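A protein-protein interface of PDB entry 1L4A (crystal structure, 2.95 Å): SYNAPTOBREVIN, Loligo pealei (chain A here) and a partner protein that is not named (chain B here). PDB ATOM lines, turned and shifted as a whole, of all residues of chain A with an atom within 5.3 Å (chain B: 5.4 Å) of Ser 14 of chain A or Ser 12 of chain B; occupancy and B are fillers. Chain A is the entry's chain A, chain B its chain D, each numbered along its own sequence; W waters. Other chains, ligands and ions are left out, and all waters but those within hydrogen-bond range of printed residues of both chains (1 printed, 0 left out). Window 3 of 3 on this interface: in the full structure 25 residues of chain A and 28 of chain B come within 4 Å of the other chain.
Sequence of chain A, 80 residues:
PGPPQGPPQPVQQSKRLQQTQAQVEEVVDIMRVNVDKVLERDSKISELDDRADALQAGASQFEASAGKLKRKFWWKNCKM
Ser 14 of chain A touches one residue of chain B. Of chain A, only Ser 14 (2.8 Å), Lys 15 (2.8 Å) and Arg 16 (3.1 Å) come within 4 Å of Ser 12 of chain B. Of the printed residues of chain B, Lys 15 of chain A touches Pro 11 and Ser 12. Of the printed residues of chain A, Ser 13 of chain B touches Arg 16. The nearest residue of chain B that does not touch Ser 14 of chain A is Pro 11 of chain B (4.2 Å). The nearest residue of chain A that does not touch Ser 12 of chain B is Gln 13 of chain A (4.1 Å). The nearest printed residue of chain A that does not touch Tyr 15 of chain B is Lys 15 of chain A (6.3 Å).
The backbone NH (N) of Leu 17 of chain A lies within hydrogen-bond range of the backbone carbonyl oxygen (O) of Pro 11 of chain B, 3.4 Å away. The guanidinium group of Arg 16 of chain A is in hydrogen-bond range of the side-chain hydroxyl of Tyr 15 of chain B, 3.3 Å away.
Among the printed residues, pairs that only touch across the chains: Ser 14 of chain A with Ser 12 of chain B (2.8 Å), Lys 15 of chain A with Ser 12 of chain B (2.8 Å), Arg 16 of chain A with Ser 12 of chain B (3.1 Å), Lys 15 of chain A with Pro 11 of chain B (3.2 Å), Arg 16 of chain A with Pro 11 of chain B (3.6 Å), Arg 16 of chain A with Ser 13 of chain B (3.8 Å) and Leu 17 of chain A with Tyr 15 of chain B (3.9 Å).
Water W1 bridges the backbone NH of Ser 12 of chain B (2.5 Å) and the backbone carbonyl oxygen of Ser 14 of chain A (2.6 Å).
Of the 6 printed residues of chain A, 4 touch a printed residue of chain B. Hydrophobic or aromatic side chains of chain A that line the printed part of chain B: Leu 17. Among the printed residues, no Asp or Glu carboxylate lies within 4 Å of a Lys or Arg side-chain nitrogen of the other chain.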
ATOM      1  N   GLN A  12     -13.269  20.999  21.725  1.00  0.00           N
ATOM      2  CA  GLN A  12     -12.726  21.042  20.366  1.00  0.00           C
ATOM      3  C   GLN A  12     -13.950  20.909  19.465  1.00  0.00           C
ATOM      4  O   GLN A  12     -14.761  20.013  19.669  1.00  0.00           O
ATOM      5  CB  GLN A  12     -11.779  19.864  20.119  1.00  0.00           C
ATOM      6  CG  GLN A  12     -10.921  20.003  18.866  1.00  0.00           C
ATOM      7  CD  GLN A  12      -9.709  20.893  19.085  1.00  0.00           C
ATOM      8  OE1 GLN A  12      -9.811  21.949  19.702  1.00  0.00           O
ATOM      9  NE2 GLN A  12      -8.559  20.474  18.571  1.00  0.00           N
ATOM     10  N   GLN A  13     -14.097  21.786  18.476  1.00  0.00           N
ATOM     11  CA  GLN A  13     -15.275  21.728  17.613  1.00  0.00           C
ATOM     12  C   GLN A  13     -15.179  22.381  16.233  1.00  0.00           C
ATOM     13  O   GLN A  13     -15.984  23.247  15.895  1.00  0.00           O
ATOM     14  CB  GLN A  13     -16.495  22.297  18.365  1.00  0.00           C
ATOM     15  CG  GLN A  13     -16.192  23.227  19.537  1.00  0.00           C
ATOM     16  CD  GLN A  13     -15.640  24.577  19.101  1.00  0.00           C
ATOM     17  OE1 GLN A  13     -16.307  25.325  18.387  1.00  0.00           O
ATOM     18  NE2 GLN A  13     -14.418  24.900  19.533  1.00  0.00           N
ATOM     19  N   SER A  14     -14.221  21.939  15.425  1.00  0.00           N
ATOM     20  CA  SER A  14     -14.059  22.510  14.097  1.00  0.00           C
ATOM     21  C   SER A  14     -13.742  21.487  13.013  1.00  0.00           C
ATOM     22  O   SER A  14     -14.012  21.727  11.830  1.00  0.00           O
ATOM     23  CB  SER A  14     -12.958  23.566  14.116  1.00  0.00           C
ATOM     24  OG  SER A  14     -11.767  23.027  14.651  1.00  0.00           O
ATOM     25  N   LYS A  15     -13.175  20.351  13.406  1.00  0.00           N
ATOM     26  CA  LYS A  15     -12.830  19.318  12.447  1.00  0.00           C
ATOM     27  C   LYS A  15     -12.672  18.017  13.202  1.00  0.00           C
ATOM     28  O   LYS A  15     -11.621  17.353  13.165  1.00  0.00           O
ATOM     29  CB  LYS A  15     -11.539  19.684  11.726  1.00  0.00           C
ATOM     30  CG  LYS A  15     -11.642  20.919  10.838  1.00  0.00           C
ATOM     31  CD  LYS A  15     -11.391  20.593   9.395  1.00  0.00           C
ATOM     32  CE  LYS A  15     -11.768  21.772   8.530  1.00  0.00           C
ATOM     33  NZ  LYS A  15     -11.555  21.491   7.071  1.00  0.00           N
ATOM     34  N   ARG A  16     -13.762  17.670  13.881  1.00  0.00           N
ATOM     35  CA  ARG A  16     -13.873  16.479  14.704  1.00  0.00           C
ATOM     36  C   ARG A  16     -13.412  15.223  13.995  1.00  0.00           C
ATOM     37  O   ARG A  16     -12.990  14.261  14.652  1.00  0.00           O
ATOM     38  CB  ARG A  16     -15.307  16.331  15.167  1.00  0.00           C
ATOM     39  CG  ARG A  16     -15.951  17.677  15.432  1.00  0.00           C
ATOM     40  CD  ARG A  16     -16.250  17.899  16.893  1.00  0.00           C
ATOM     41  NE  ARG A  16     -17.619  17.514  17.229  1.00  0.00           N
ATOM     42  CZ  ARG A  16     -17.922  16.528  18.063  1.00  0.00           C
ATOM     43  NH1 ARG A  16     -16.958  15.830  18.636  1.00  0.00           N
ATOM     44  NH2 ARG A  16     -19.184  16.251  18.336  1.00  0.00           N
ATOM     45  N   LEU A  17     -13.483  15.198  12.668  1.00  0.00           N
ATOM     46  CA  LEU A  17     -12.995  14.004  11.999  1.00  0.00           C
ATOM     47  C   LEU A  17     -11.490  13.978  12.160  1.00  0.00           C
ATOM     48  O   LEU A  17     -10.932  13.061  12.783  1.00  0.00           O
ATOM     49  CB  LEU A  17     -13.342  13.998  10.518  1.00  0.00           C
ATOM     50  CG  LEU A  17     -13.406  12.606   9.869  1.00  0.00           C
ATOM     51  CD1 LEU A  17     -13.987  11.606  10.861  1.00  0.00           C
ATOM     52  CD2 LEU A  17     -14.270  12.655   8.601  1.00  0.00           C
ATOM     53  N   PRO B  11     -15.544  19.794   8.461  1.00  0.00           N
ATOM     54  CA  PRO B  11     -15.625  18.373   8.826  1.00  0.00           C
ATOM     55  C   PRO B  11     -15.937  18.164  10.310  1.00  0.00           C
ATOM     56  O   PRO B  11     -15.601  17.118  10.894  1.00  0.00           O
ATOM     57  CB  PRO B  11     -14.253  17.846   8.435  1.00  0.00           C
ATOM     58  CG  PRO B  11     -13.919  18.677   7.215  1.00  0.00           C
ATOM     59  CD  PRO B  11     -14.371  20.063   7.609  1.00  0.00           C
ATOM     60  N   SER B  12     -16.573  19.179  10.903  1.00  0.00           N
ATOM     61  CA  SER B  12     -16.957  19.168  12.312  1.00  0.00           C
ATOM     62  C   SER B  12     -18.250  19.902  12.600  1.00  0.00           C
ATOM     63  O   SER B  12     -18.944  20.353  11.684  1.00  0.00           O
ATOM     64  CB  SER B  12     -15.885  19.741  13.143  1.00  0.00           C
ATOM     65  N   SER B  13     -18.534  20.057  13.891  1.00  0.00           N
ATOM     66  CA  SER B  13     -19.788  20.641  14.352  1.00  0.00           C
ATOM     67  C   SER B  13     -20.670  19.417  14.096  1.00  0.00           C
ATOM     68  O   SER B  13     -21.888  19.497  13.970  1.00  0.00           O
ATOM     69  CB  SER B  13     -20.218  21.816  13.465  1.00  0.00           C
ATOM     70  OG  SER B  13     -21.398  22.448  13.947  1.00  0.00           O
ATOM     71  N   GLY B  14     -19.979  18.280  14.033  1.00  0.00           N
ATOM     72  CA  GLY B  14     -20.554  16.981  13.765  1.00  0.00           C
ATOM     73  C   GLY B  14     -19.479  16.324  12.917  1.00  0.00           C
ATOM     74  O   GLY B  14     -19.116  16.865  11.878  1.00  0.00           O
ATOM     75  N   TYR B  15     -18.944  15.184  13.345  1.00  0.00           N
ATOM     76  CA  TYR B  15     -17.896  14.528  12.572  1.00  0.00           C
ATOM     77  C   TYR B  15     -18.212  14.371  11.089  1.00  0.00           C
ATOM     78  O   TYR B  15     -17.308  14.402  10.253  1.00  0.00           O
ATOM     79  CB  TYR B  15     -17.600  13.141  13.115  1.00  0.00           C
ATOM     80  CG  TYR B  15     -17.406  13.058  14.597  1.00  0.00           C
ATOM     81  CD1 TYR B  15     -18.483  13.177  15.466  1.00  0.00           C
ATOM     82  CD2 TYR B  15     -16.154  12.784  15.132  1.00  0.00           C
ATOM     83  CE1 TYR B  15     -18.323  13.011  16.825  1.00  0.00           C
ATOM     84  CE2 TYR B  15     -15.981  12.624  16.490  1.00  0.00           C
ATOM     85  CZ  TYR B  15     -17.066  12.732  17.331  1.00  0.00           C
ATOM     86  OH  TYR B  15     -16.895  12.532  18.683  1.00  0.00           O
ATOM     87  N   THR B  17     -20.028  15.711   7.670  1.00  0.00           N
ATOM     88  CA  THR B  17     -20.603  16.842   6.951  1.00  0.00           C
ATOM     89  C   THR B  17     -21.764  16.438   6.043  1.00  0.00           C
ATOM     90  O   THR B  17     -21.589  15.833   4.979  1.00  0.00           O
ATOM     91  CB  THR B  17     -19.506  17.591   6.142  1.00  0.00           C
ATOM     92  OG1 THR B  17     -18.730  18.395   7.041  1.00  0.00           O
ATOM     93  CG2 THR B  17     -20.111  18.486   5.068  1.00  0.00           C
HETATM   94  O   HOH W   1     -16.192  21.593  10.465  1.00  0.00           O
